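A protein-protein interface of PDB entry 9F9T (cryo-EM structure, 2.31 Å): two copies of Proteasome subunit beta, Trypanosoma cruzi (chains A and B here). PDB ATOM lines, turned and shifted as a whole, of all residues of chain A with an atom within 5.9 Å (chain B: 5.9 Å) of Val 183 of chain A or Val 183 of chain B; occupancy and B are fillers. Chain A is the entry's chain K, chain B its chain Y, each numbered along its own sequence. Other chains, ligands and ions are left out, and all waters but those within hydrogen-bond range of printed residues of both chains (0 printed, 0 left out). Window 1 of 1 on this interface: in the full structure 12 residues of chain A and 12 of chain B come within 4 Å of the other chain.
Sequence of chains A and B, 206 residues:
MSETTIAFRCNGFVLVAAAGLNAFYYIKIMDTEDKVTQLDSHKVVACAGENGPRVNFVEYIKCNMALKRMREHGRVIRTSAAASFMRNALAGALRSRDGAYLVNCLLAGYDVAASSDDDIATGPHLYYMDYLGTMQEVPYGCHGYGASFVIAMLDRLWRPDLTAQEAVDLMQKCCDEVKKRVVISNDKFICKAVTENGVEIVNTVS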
ATOM      1  N   LEU A  21      -4.502 -33.331  -4.092  1.00  0.00           N
ATOM      2  CA  LEU A  21      -3.691 -32.468  -3.249  1.00  0.00           C
ATOM      3  C   LEU A  21      -4.321 -32.023  -1.928  1.00  0.00           C
ATOM      4  O   LEU A  21      -5.385 -31.464  -1.888  1.00  0.00           O
ATOM      5  CB  LEU A  21      -3.343 -31.227  -4.081  1.00  0.00           C
ATOM      6  CG  LEU A  21      -2.657 -30.116  -3.291  1.00  0.00           C
ATOM      7  CD1 LEU A  21      -1.201 -30.452  -3.082  1.00  0.00           C
ATOM      8  CD2 LEU A  21      -2.797 -28.771  -3.958  1.00  0.00           C
ATOM      9  N   ASN A  22      -3.555 -32.149  -0.851  1.00  0.00           N
ATOM     10  CA  ASN A  22      -3.829 -31.491   0.422  1.00  0.00           C
ATOM     11  C   ASN A  22      -2.574 -30.715   0.859  1.00  0.00           C
ATOM     12  O   ASN A  22      -1.461 -31.247   0.933  1.00  0.00           O
ATOM     13  CB  ASN A  22      -4.283 -32.526   1.475  1.00  0.00           C
ATOM     14  CG  ASN A  22      -4.652 -31.886   2.793  1.00  0.00           C
ATOM     15  OD1 ASN A  22      -3.859 -31.176   3.396  1.00  0.00           O
ATOM     16  ND2 ASN A  22      -5.865 -32.119   3.260  1.00  0.00           N
ATOM     17  N   ALA A  23      -2.770 -29.449   1.169  1.00  0.00           N
ATOM     18  CA  ALA A  23      -1.684 -28.495   1.294  1.00  0.00           C
ATOM     19  C   ALA A  23      -1.831 -27.753   2.609  1.00  0.00           C
ATOM     20  O   ALA A  23      -2.945 -27.514   3.019  1.00  0.00           O
ATOM     21  CB  ALA A  23      -1.768 -27.463   0.167  1.00  0.00           C
ATOM     22  N   PHE A  24      -0.707 -27.311   3.182  1.00  0.00           N
ATOM     23  CA  PHE A  24      -0.702 -26.389   4.302  1.00  0.00           C
ATOM     24  C   PHE A  24       0.113 -25.191   3.832  1.00  0.00           C
ATOM     25  O   PHE A  24       1.325 -25.243   3.714  1.00  0.00           O
ATOM     26  CB  PHE A  24      -0.255 -27.140   5.575  1.00  0.00           C
ATOM     27  CG  PHE A  24      -0.143 -26.317   6.833  1.00  0.00           C
ATOM     28  CD1 PHE A  24      -1.125 -26.379   7.819  1.00  0.00           C
ATOM     29  CD2 PHE A  24       0.941 -25.463   7.041  1.00  0.00           C
ATOM     30  CE1 PHE A  24      -1.040 -25.592   8.967  1.00  0.00           C
ATOM     31  CE2 PHE A  24       1.026 -24.676   8.189  1.00  0.00           C
ATOM     32  CZ  PHE A  24       0.035 -24.742   9.151  1.00  0.00           C
ATOM     33  N   TYR A  25      -0.585 -24.109   3.515  1.00  0.00           N
ATOM     34  CA  TYR A  25       0.018 -22.961   2.870  1.00  0.00           C
ATOM     35  C   TYR A  25       0.744 -23.463   1.622  1.00  0.00           C
ATOM     36  O   TYR A  25       0.137 -24.120   0.770  1.00  0.00           O
ATOM     37  CB  TYR A  25       0.874 -22.177   3.865  1.00  0.00           C
ATOM     38  CG  TYR A  25       0.087 -21.570   5.009  1.00  0.00           C
ATOM     39  CD1 TYR A  25      -0.723 -20.453   4.813  1.00  0.00           C
ATOM     40  CD2 TYR A  25       0.138 -22.124   6.286  1.00  0.00           C
ATOM     41  CE1 TYR A  25      -1.449 -19.900   5.859  1.00  0.00           C
ATOM     42  CE2 TYR A  25      -0.581 -21.580   7.339  1.00  0.00           C
ATOM     43  CZ  TYR A  25      -1.378 -20.466   7.124  1.00  0.00           C
ATOM     44  OH  TYR A  25      -2.091 -19.925   8.157  1.00  0.00           O
ATOM     45  N   TYR A  26       2.043 -23.180   1.510  1.00  0.00           N
ATOM     46  CA  TYR A  26       2.725 -23.606   0.314  1.00  0.00           C
ATOM     47  C   TYR A  26       3.202 -25.056   0.418  1.00  0.00           C
ATOM     48  O   TYR A  26       3.711 -25.600  -0.543  1.00  0.00           O
ATOM     49  CB  TYR A  26       3.754 -22.527   0.008  1.00  0.00           C
ATOM     50  CG  TYR A  26       4.798 -22.317   1.088  1.00  0.00           C
ATOM     51  CD1 TYR A  26       5.935 -23.136   1.167  1.00  0.00           C
ATOM     52  CD2 TYR A  26       4.662 -21.297   2.014  1.00  0.00           C
ATOM     53  CE1 TYR A  26       6.886 -22.959   2.162  1.00  0.00           C
ATOM     54  CE2 TYR A  26       5.604 -21.120   3.017  1.00  0.00           C
ATOM     55  CZ  TYR A  26       6.717 -21.948   3.096  1.00  0.00           C
ATOM     56  OH  TYR A  26       7.656 -21.733   4.063  1.00  0.00           O
ATOM     57  N   ILE A  27       3.063 -25.700   1.543  1.00  0.00           N
ATOM     58  CA  ILE A  27       3.655 -27.015   1.672  1.00  0.00           C
ATOM     59  C   ILE A  27       2.661 -28.067   1.181  1.00  0.00           C
ATOM     60  O   ILE A  27       1.570 -28.126   1.682  1.00  0.00           O
ATOM     61  CB  ILE A  27       4.119 -27.266   3.141  1.00  0.00           C
ATOM     62  CG1 ILE A  27       5.166 -26.251   3.610  1.00  0.00           C
ATOM     63  CG2 ILE A  27       4.701 -28.678   3.315  1.00  0.00           C
ATOM     64  CD1 ILE A  27       4.619 -25.054   4.403  1.00  0.00           C
ATOM     65  N   LYS A  28       3.079 -29.021   0.364  1.00  0.00           N
ATOM     66  CA  LYS A  28       2.259 -30.187   0.080  1.00  0.00           C
ATOM     67  C   LYS A  28       2.281 -31.226   1.200  1.00  0.00           C
ATOM     68  O   LYS A  28       3.239 -31.969   1.344  1.00  0.00           O
ATOM     69  CB  LYS A  28       2.744 -30.920  -1.165  1.00  0.00           C
ATOM     70  CG  LYS A  28       2.340 -30.247  -2.447  1.00  0.00           C
ATOM     71  CD  LYS A  28       2.943 -30.827  -3.694  1.00  0.00           C
ATOM     72  CE  LYS A  28       2.370 -32.161  -4.092  1.00  0.00           C
ATOM     73  NZ  LYS A  28       2.811 -32.469  -5.479  1.00  0.00           N
ATOM     74  N   VAL A 178      -4.937 -29.084 -16.848  1.00  0.00           N
ATOM     75  CA  VAL A 178      -4.850 -28.507 -15.523  1.00  0.00           C
ATOM     76  C   VAL A 178      -3.422 -28.511 -14.989  1.00  0.00           C
ATOM     77  O   VAL A 178      -2.998 -27.474 -14.458  1.00  0.00           O
ATOM     78  CB  VAL A 178      -5.806 -29.242 -14.584  1.00  0.00           C
ATOM     79  CG1 VAL A 178      -5.554 -28.883 -13.131  1.00  0.00           C
ATOM     80  CG2 VAL A 178      -7.224 -28.913 -15.025  1.00  0.00           C
ATOM     81  N   ARG A 181      -1.178 -25.902 -16.942  1.00  0.00           N
ATOM     82  CA  ARG A 181      -1.386 -24.462 -16.931  1.00  0.00           C
ATOM     83  C   ARG A 181      -1.712 -23.871 -15.572  1.00  0.00           C
ATOM     84  O   ARG A 181      -1.791 -22.657 -15.454  1.00  0.00           O
ATOM     85  CB  ARG A 181      -2.585 -24.100 -17.810  1.00  0.00           C
ATOM     86  CG  ARG A 181      -2.350 -24.192 -19.298  1.00  0.00           C
ATOM     87  CD  ARG A 181      -1.520 -22.969 -19.707  1.00  0.00           C
ATOM     88  NE  ARG A 181      -1.004 -23.269 -21.041  1.00  0.00           N
ATOM     89  CZ  ARG A 181       0.086 -22.748 -21.551  1.00  0.00           C
ATOM     90  NH1 ARG A 181       0.787 -21.867 -20.870  1.00  0.00           N
ATOM     91  NH2 ARG A 181       0.436 -23.077 -22.780  1.00  0.00           N
ATOM     92  N   VAL A 182      -1.980 -24.688 -14.565  1.00  0.00           N
ATOM     93  CA  VAL A 182      -2.253 -24.148 -13.245  1.00  0.00           C
ATOM     94  C   VAL A 182      -0.997 -24.271 -12.406  1.00  0.00           C
ATOM     95  O   VAL A 182      -0.302 -25.282 -12.434  1.00  0.00           O
ATOM     96  CB  VAL A 182      -3.465 -24.822 -12.591  1.00  0.00           C
ATOM     97  CG1 VAL A 182      -3.686 -24.347 -11.173  1.00  0.00           C
ATOM     98  CG2 VAL A 182      -4.723 -24.584 -13.380  1.00  0.00           C
ATOM     99  N   VAL A 183      -0.694 -23.176 -11.731  1.00  0.00           N
ATOM    100  CA  VAL A 183       0.554 -22.991 -11.005  1.00  0.00           C
ATOM    101  C   VAL A 183       0.515 -23.802  -9.710  1.00  0.00           C
ATOM    102  O   VAL A 183       1.443 -24.545  -9.443  1.00  0.00           O
ATOM    103  CB  VAL A 183       0.810 -21.487 -10.779  1.00  0.00           C
ATOM    104  CG1 VAL A 183       1.467 -21.162  -9.461  1.00  0.00           C
ATOM    105  CG2 VAL A 183       1.641 -20.929 -11.907  1.00  0.00           C
ATOM    106  N   ILE A 184      -0.549 -23.699  -8.939  1.00  0.00           N
ATOM    107  CA  ILE A 184      -0.830 -24.710  -7.930  1.00  0.00           C
ATOM    108  C   ILE A 184      -0.718 -26.052  -8.596  1.00  0.00           C
ATOM    109  O   ILE A 184      -1.254 -26.210  -9.693  1.00  0.00           O
ATOM    110  CB  ILE A 184      -2.238 -24.568  -7.356  1.00  0.00           C
ATOM    111  CG1 ILE A 184      -2.519 -23.144  -6.867  1.00  0.00           C
ATOM    112  CG2 ILE A 184      -2.444 -25.610  -6.287  1.00  0.00           C
ATOM    113  CD1 ILE A 184      -1.438 -22.564  -5.997  1.00  0.00           C
ATOM    114  N   SER A 185      -0.057 -27.001  -7.926  1.00  0.00           N
ATOM    115  CA  SER A 185       0.185 -28.328  -8.492  1.00  0.00           C
ATOM    116  C   SER A 185      -0.979 -29.245  -8.140  1.00  0.00           C
ATOM    117  O   SER A 185      -1.187 -29.560  -6.971  1.00  0.00           O
ATOM    118  CB  SER A 185       1.474 -28.949  -8.011  1.00  0.00           C
ATOM    119  OG  SER A 185       1.918 -29.968  -8.916  1.00  0.00           O
ATOM    120  N   LEU B  21       9.931 -21.510 -14.060  1.00  0.00           N
ATOM    121  CA  LEU B  21       8.569 -21.005 -14.083  1.00  0.00           C
ATOM    122  C   LEU B  21       8.406 -19.492 -14.226  1.00  0.00           C
ATOM    123  O   LEU B  21       8.932 -18.720 -13.467  1.00  0.00           O
ATOM    124  CB  LEU B  21       7.901 -21.459 -12.778  1.00  0.00           C
ATOM    125  CG  LEU B  21       6.522 -20.854 -12.536  1.00  0.00           C
ATOM    126  CD1 LEU B  21       5.490 -21.566 -13.375  1.00  0.00           C
ATOM    127  CD2 LEU B  21       6.131 -20.886 -11.081  1.00  0.00           C
ATOM    128  N   ASN B  22       7.528 -19.090 -15.138  1.00  0.00           N
ATOM    129  CA  ASN B  22       6.988 -17.735 -15.202  1.00  0.00           C
ATOM    130  C   ASN B  22       5.452 -17.814 -15.221  1.00  0.00           C
ATOM    131  O   ASN B  22       4.838 -18.513 -16.033  1.00  0.00           O
ATOM    132  CB  ASN B  22       7.560 -16.987 -16.426  1.00  0.00           C
ATOM    133  CG  ASN B  22       7.090 -15.553 -16.499  1.00  0.00           C
ATOM    134  OD1 ASN B  22       5.898 -15.278 -16.509  1.00  0.00           O
ATOM    135  ND2 ASN B  22       8.017 -14.613 -16.542  1.00  0.00           N
ATOM    136  N   ALA B  23       4.835 -17.070 -14.325  1.00  0.00           N
ATOM    137  CA  ALA B  23       3.437 -17.250 -13.984  1.00  0.00           C
ATOM    138  C   ALA B  23       2.738 -15.904 -14.044  1.00  0.00           C
ATOM    139  O   ALA B  23       3.353 -14.916 -13.710  1.00  0.00           O
ATOM    140  CB  ALA B  23       3.315 -17.772 -12.552  1.00  0.00           C
ATOM    141  N   PHE B  24       1.439 -15.911 -14.358  1.00  0.00           N
ATOM    142  CA  PHE B  24       0.588 -14.744 -14.222  1.00  0.00           C
ATOM    143  C   PHE B  24      -0.538 -15.172 -13.289  1.00  0.00           C
ATOM    144  O   PHE B  24      -1.424 -15.924 -13.654  1.00  0.00           O
ATOM    145  CB  PHE B  24       0.230 -14.212 -15.626  1.00  0.00           C
ATOM    146  CG  PHE B  24      -0.696 -13.022 -15.676  1.00  0.00           C
ATOM    147  CD1 PHE B  24      -0.205 -11.744 -15.931  1.00  0.00           C
ATOM    148  CD2 PHE B  24      -2.067 -13.167 -15.459  1.00  0.00           C
ATOM    149  CE1 PHE B  24      -1.055 -10.639 -15.942  1.00  0.00           C
ATOM    150  CE2 PHE B  24      -2.916 -12.063 -15.471  1.00  0.00           C
ATOM    151  CZ  PHE B  24      -2.409 -10.799 -15.713  1.00  0.00           C
ATOM    152  N   TYR B  25      -0.461 -14.714 -12.048  1.00  0.00           N
ATOM    153  CA  TYR B  25      -1.337 -15.183 -10.995  1.00  0.00           C
ATOM    154  C   TYR B  25      -1.242 -16.709 -10.962  1.00  0.00           C
ATOM    155  O   TYR B  25      -0.145 -17.260 -10.829  1.00  0.00           O
ATOM    156  CB  TYR B  25      -2.743 -14.608 -11.174  1.00  0.00           C
ATOM    157  CG  TYR B  25      -2.811 -13.099 -11.047  1.00  0.00           C
ATOM    158  CD1 TYR B  25      -2.709 -12.477  -9.804  1.00  0.00           C
ATOM    159  CD2 TYR B  25      -2.960 -12.293 -12.172  1.00  0.00           C
ATOM    160  CE1 TYR B  25      -2.764 -11.094  -9.687  1.00  0.00           C
ATOM    161  CE2 TYR B  25      -3.019 -10.912 -12.068  1.00  0.00           C
ATOM    162  CZ  TYR B  25      -2.919 -10.311 -10.823  1.00  0.00           C
ATOM    163  OH  TYR B  25      -2.974  -8.950 -10.711  1.00  0.00           O
ATOM    164  N   TYR B  26      -2.377 -17.398 -11.096  1.00  0.00           N
ATOM    165  CA  TYR B  26      -2.308 -18.834 -11.020  1.00  0.00           C
ATOM    166  C   TYR B  26      -1.947 -19.458 -12.369  1.00  0.00           C
ATOM    167  O   TYR B  26      -1.752 -20.656 -12.453  1.00  0.00           O
ATOM    168  CB  TYR B  26      -3.591 -19.282 -10.335  1.00  0.00           C
ATOM    169  CG  TYR B  26      -4.868 -18.920 -11.072  1.00  0.00           C
ATOM    170  CD1 TYR B  26      -5.350 -19.718 -12.121  1.00  0.00           C
ATOM    171  CD2 TYR B  26      -5.597 -17.801 -10.712  1.00  0.00           C
ATOM    172  CE1 TYR B  26      -6.508 -19.385 -12.809  1.00  0.00           C
ATOM    173  CE2 TYR B  26      -6.751 -17.455 -11.402  1.00  0.00           C
ATOM    174  CZ  TYR B  26      -7.209 -18.243 -12.451  1.00  0.00           C
ATOM    175  OH  TYR B  26      -8.369 -17.913 -13.091  1.00  0.00           O
ATOM    176  N   ILE B  27      -1.854 -18.699 -13.424  1.00  0.00           N
ATOM    177  CA  ILE B  27      -1.663 -19.322 -14.717  1.00  0.00           C
ATOM    178  C   ILE B  27      -0.168 -19.511 -14.972  1.00  0.00           C
ATOM    179  O   ILE B  27       0.560 -18.555 -14.934  1.00  0.00           O
ATOM    180  CB  ILE B  27      -2.363 -18.490 -15.836  1.00  0.00           C
ATOM    181  CG1 ILE B  27      -3.875 -18.360 -15.617  1.00  0.00           C
ATOM    182  CG2 ILE B  27      -2.127 -19.103 -17.227  1.00  0.00           C
ATOM    183  CD1 ILE B  27      -4.333 -17.070 -14.917  1.00  0.00           C
ATOM    184  N   LYS B  28       0.270 -20.674 -15.426  1.00  0.00           N
ATOM    185  CA  LYS B  28       1.624 -20.826 -15.935  1.00  0.00           C
ATOM    186  C   LYS B  28       1.802 -20.279 -17.349  1.00  0.00           C
ATOM    187  O   LYS B  28       1.397 -20.906 -18.316  1.00  0.00           O
ATOM    188  CB  LYS B  28       2.028 -22.295 -16.011  1.00  0.00           C
ATOM    189  CG  LYS B  28       2.397 -22.879 -14.676  1.00  0.00           C
ATOM    190  CD  LYS B  28       2.629 -24.364 -14.669  1.00  0.00           C
ATOM    191  CE  LYS B  28       3.915 -24.788 -15.327  1.00  0.00           C
ATOM    192  NZ  LYS B  28       4.171 -26.212 -14.986  1.00  0.00           N
ATOM    193  N   VAL B 178      12.084 -30.006  -3.855  1.00  0.00           N
ATOM    194  CA  VAL B 178      11.288 -28.827  -4.125  1.00  0.00           C
ATOM    195  C   VAL B 178       9.997 -29.165  -4.865  1.00  0.00           C
ATOM    196  O   VAL B 178       8.946 -28.647  -4.462  1.00  0.00           O
ATOM    197  CB  VAL B 178      12.129 -27.810  -4.895  1.00  0.00           C
ATOM    198  CG1 VAL B 178      11.277 -26.686  -5.459  1.00  0.00           C
ATOM    199  CG2 VAL B 178      13.210 -27.302  -3.952  1.00  0.00           C
ATOM    200  N   ARG B 181       7.476 -31.079  -2.496  1.00  0.00           N
ATOM    201  CA  ARG B 181       6.870 -30.510  -1.301  1.00  0.00           C
ATOM    202  C   ARG B 181       6.378 -29.083  -1.447  1.00  0.00           C
ATOM    203  O   ARG B 181       5.759 -28.570  -0.527  1.00  0.00           O
ATOM    204  CB  ARG B 181       7.899 -30.455  -0.170  1.00  0.00           C
ATOM    205  CG  ARG B 181       8.238 -31.781   0.465  1.00  0.00           C
ATOM    206  CD  ARG B 181       7.069 -32.160   1.382  1.00  0.00           C
ATOM    207  NE  ARG B 181       7.246 -33.579   1.685  1.00  0.00           N
ATOM    208  CZ  ARG B 181       6.276 -34.396   2.013  1.00  0.00           C
ATOM    209  NH1 ARG B 181       5.039 -33.955   2.115  1.00  0.00           N
ATOM    210  NH2 ARG B 181       6.566 -35.652   2.292  1.00  0.00           N
ATOM    211  N   VAL B 182       6.702 -28.402  -2.536  1.00  0.00           N
ATOM    212  CA  VAL B 182       6.209 -27.050  -2.719  1.00  0.00           C
ATOM    213  C   VAL B 182       5.020 -27.091  -3.657  1.00  0.00           C
ATOM    214  O   VAL B 182       5.020 -27.794  -4.664  1.00  0.00           O
ATOM    215  CB  VAL B 182       7.311 -26.103  -3.207  1.00  0.00           C
ATOM    216  CG1 VAL B 182       6.780 -24.719  -3.511  1.00  0.00           C
ATOM    217  CG2 VAL B 182       8.424 -25.980  -2.204  1.00  0.00           C
ATOM    218  N   VAL B 183       3.986 -26.380  -3.246  1.00  0.00           N
ATOM    219  CA  VAL B 183       2.676 -26.412  -3.880  1.00  0.00           C
ATOM    220  C   VAL B 183       2.725 -25.623  -5.189  1.00  0.00           C
ATOM    221  O   VAL B 183       2.308 -26.138  -6.211  1.00  0.00           O
ATOM    222  CB  VAL B 183       1.605 -25.899  -2.895  1.00  0.00           C
ATOM    223  CG1 VAL B 183       0.496 -25.109  -3.546  1.00  0.00           C
ATOM    224  CG2 VAL B 183       1.016 -27.054  -2.126  1.00  0.00           C
ATOM    225  N   ILE B 184       3.260 -24.418  -5.174  1.00  0.00           N
ATOM    226  CA  ILE B 184       3.696 -23.790  -6.414  1.00  0.00           C
ATOM    227  C   ILE B 184       4.532 -24.793  -7.156  1.00  0.00           C
ATOM    228  O   ILE B 184       5.384 -25.424  -6.532  1.00  0.00           O
ATOM    229  CB  ILE B 184       4.544 -22.545  -6.156  1.00  0.00           C
ATOM    230  CG1 ILE B 184       3.854 -21.567  -5.202  1.00  0.00           C
ATOM    231  CG2 ILE B 184       4.918 -21.920  -7.474  1.00  0.00           C
ATOM    232  CD1 ILE B 184       2.419 -21.273  -5.547  1.00  0.00           C
ATOM    233  N   SER B 185       4.303 -24.910  -8.467  1.00  0.00           N
ATOM    234  CA  SER B 185       4.997 -25.899  -9.293  1.00  0.00           C
ATOM    235  C   SER B 185       6.285 -25.292  -9.829  1.00  0.00           C
ATOM    236  O   SER B 185       6.245 -24.358 -10.628  1.00  0.00           O
ATOM    237  CB  SER B 185       4.160 -26.396 -10.446  1.00  0.00           C
ATOM    238  OG  SER B 185       4.640 -27.661 -10.918  1.00  0.00           O
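The backbone carbonyl oxygen (O) of Tyr 26 of chain A is in hydrogen-bond range of the backbone NH (N) of Val 183 of chain B. NH1 of Arg 181 of chain B is in hydrogen-bond range of O of Lys 28 of chain A, 2.8 Å away. The guanidinium group of Arg 181 of chain A is in hydrogen-bond range of the backbone carbonyl oxygen of Lys 28 of chain B (2.8 Å). The backbone carbonyl oxygen of Tyr 26 of chain B is in hydrogen-bond range of the backbone NH of Val 183 of chain A, 2.8 Å away. The backbone NH (N) of Ser 185 of chain B is in hydrogen-bond range of the backbone carbonyl oxygen (O) of Val 183 of chain A (3.0 Å). The backbone NH (N) of Ser 185 of chain A is in hydrogen-bond range of the backbone carbonyl oxygen (O) of Val 183 of chain B (3.0 Å).
Among the printed residues, merely in contact across the chains: Ala 23 of chain A with Val 183 of chain B, Tyr 26 of chain A with Arg 181 of chain B, Tyr 26 of chain A with Val 182 of chain B, Ile 27 of chain A with Arg 181 of chain B, Ile 27 of chain A with Val 183 of chain B, Lys 28 of chain A with Val 182 of chain B, Lys 28 of chain A with Val 183 of chain B, Arg 181 of chain A with Tyr 26 of chain B, Arg 181 of chain A with Ile 27 of chain B, Val 182 of chain A with Tyr 26 of chain B, Val 182 of chain A with Lys 28 of chain B, Val 183 of chain A with Ala 23 of chain B, Val 183 of chain A with Ile 27 of chain B, Val 183 of chain A with Lys 28 of chain B, Val 183 of chain A with Val 183 of chain B, Val 183 of chain A with Ile 184 of chain B and Ile 184 of chain A with Val 183 of chain B.
Asn 22 of chain A touches none of the printed residues of chain B. Of the printed residues of chain B, Arg 181 of chain A touches Tyr 26 (3.6 Å), Ile 27 (3.4 Å) and Lys 28 (2.8 Å). Of the printed residues of chain B, Ile 184 of chain A touches Val 183. Printed residues of chain B within 4 Å of Ser 185 of chain A: Val 183 (3.0 Å). Asn 22 of chain B touches none of the printed residues of chain A. Printed residues of chain A within 4 Å of Val 182 of chain B: Tyr 26 and Lys 28. Of chain A, only Ala 23, Tyr 26, Ile 27, Lys 28, Val 183, Ile 184 and Ser 185 come within 4 Å of Val 183 of chain B. Printed residues of chain A within 4 Å of Ser 185 of chain B: Val 183. The nearest residue of chain B that does not touch Val 183 of chain A is Leu 21 of chain B (4.2 Å). The nearest residue of chain A that does not touch Val 183 of chain B is Leu 21 of chain A (4.2 Å). The nearest printed residue of chain B that does not touch Arg 181 of chain A is Phe 24 of chain B (7.0 Å).
Hydrophobic or aromatic side chains of chain B within 4 Å of the printed part of chain A: Ala 23, Ile 27 and Val 183. Of the 14 printed residues of chain A, 9 touch a printed residue of chain B. Among the printed residues, 23 pairs touch across the chains.
Ala 23 of chain A touches Val 183 of chain B, and with the chains exchanged Val 183 of chain A touches Ala 23 of chain B. Lys 28 of chain A touches Arg 181 of chain B, and with the chains exchanged Arg 181 of chain A touches Lys 28 of chain B. Lys 28 of chain A touches Val 182 of chain B, and with the chains exchanged Val 182 of chain A touches Lys 28 of chain B. Val 183 of chain A touches its own counterpart, Val 183 of chain B. Positions printed for both chains: 21, 22, 23, 24, 25, 26, 27, 28, 178, 181, 182, 183, 184 and 185. Of the 23 pairs that touch across the chains among the printed residues, 23 have their exchanged pair printed and touching as well.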
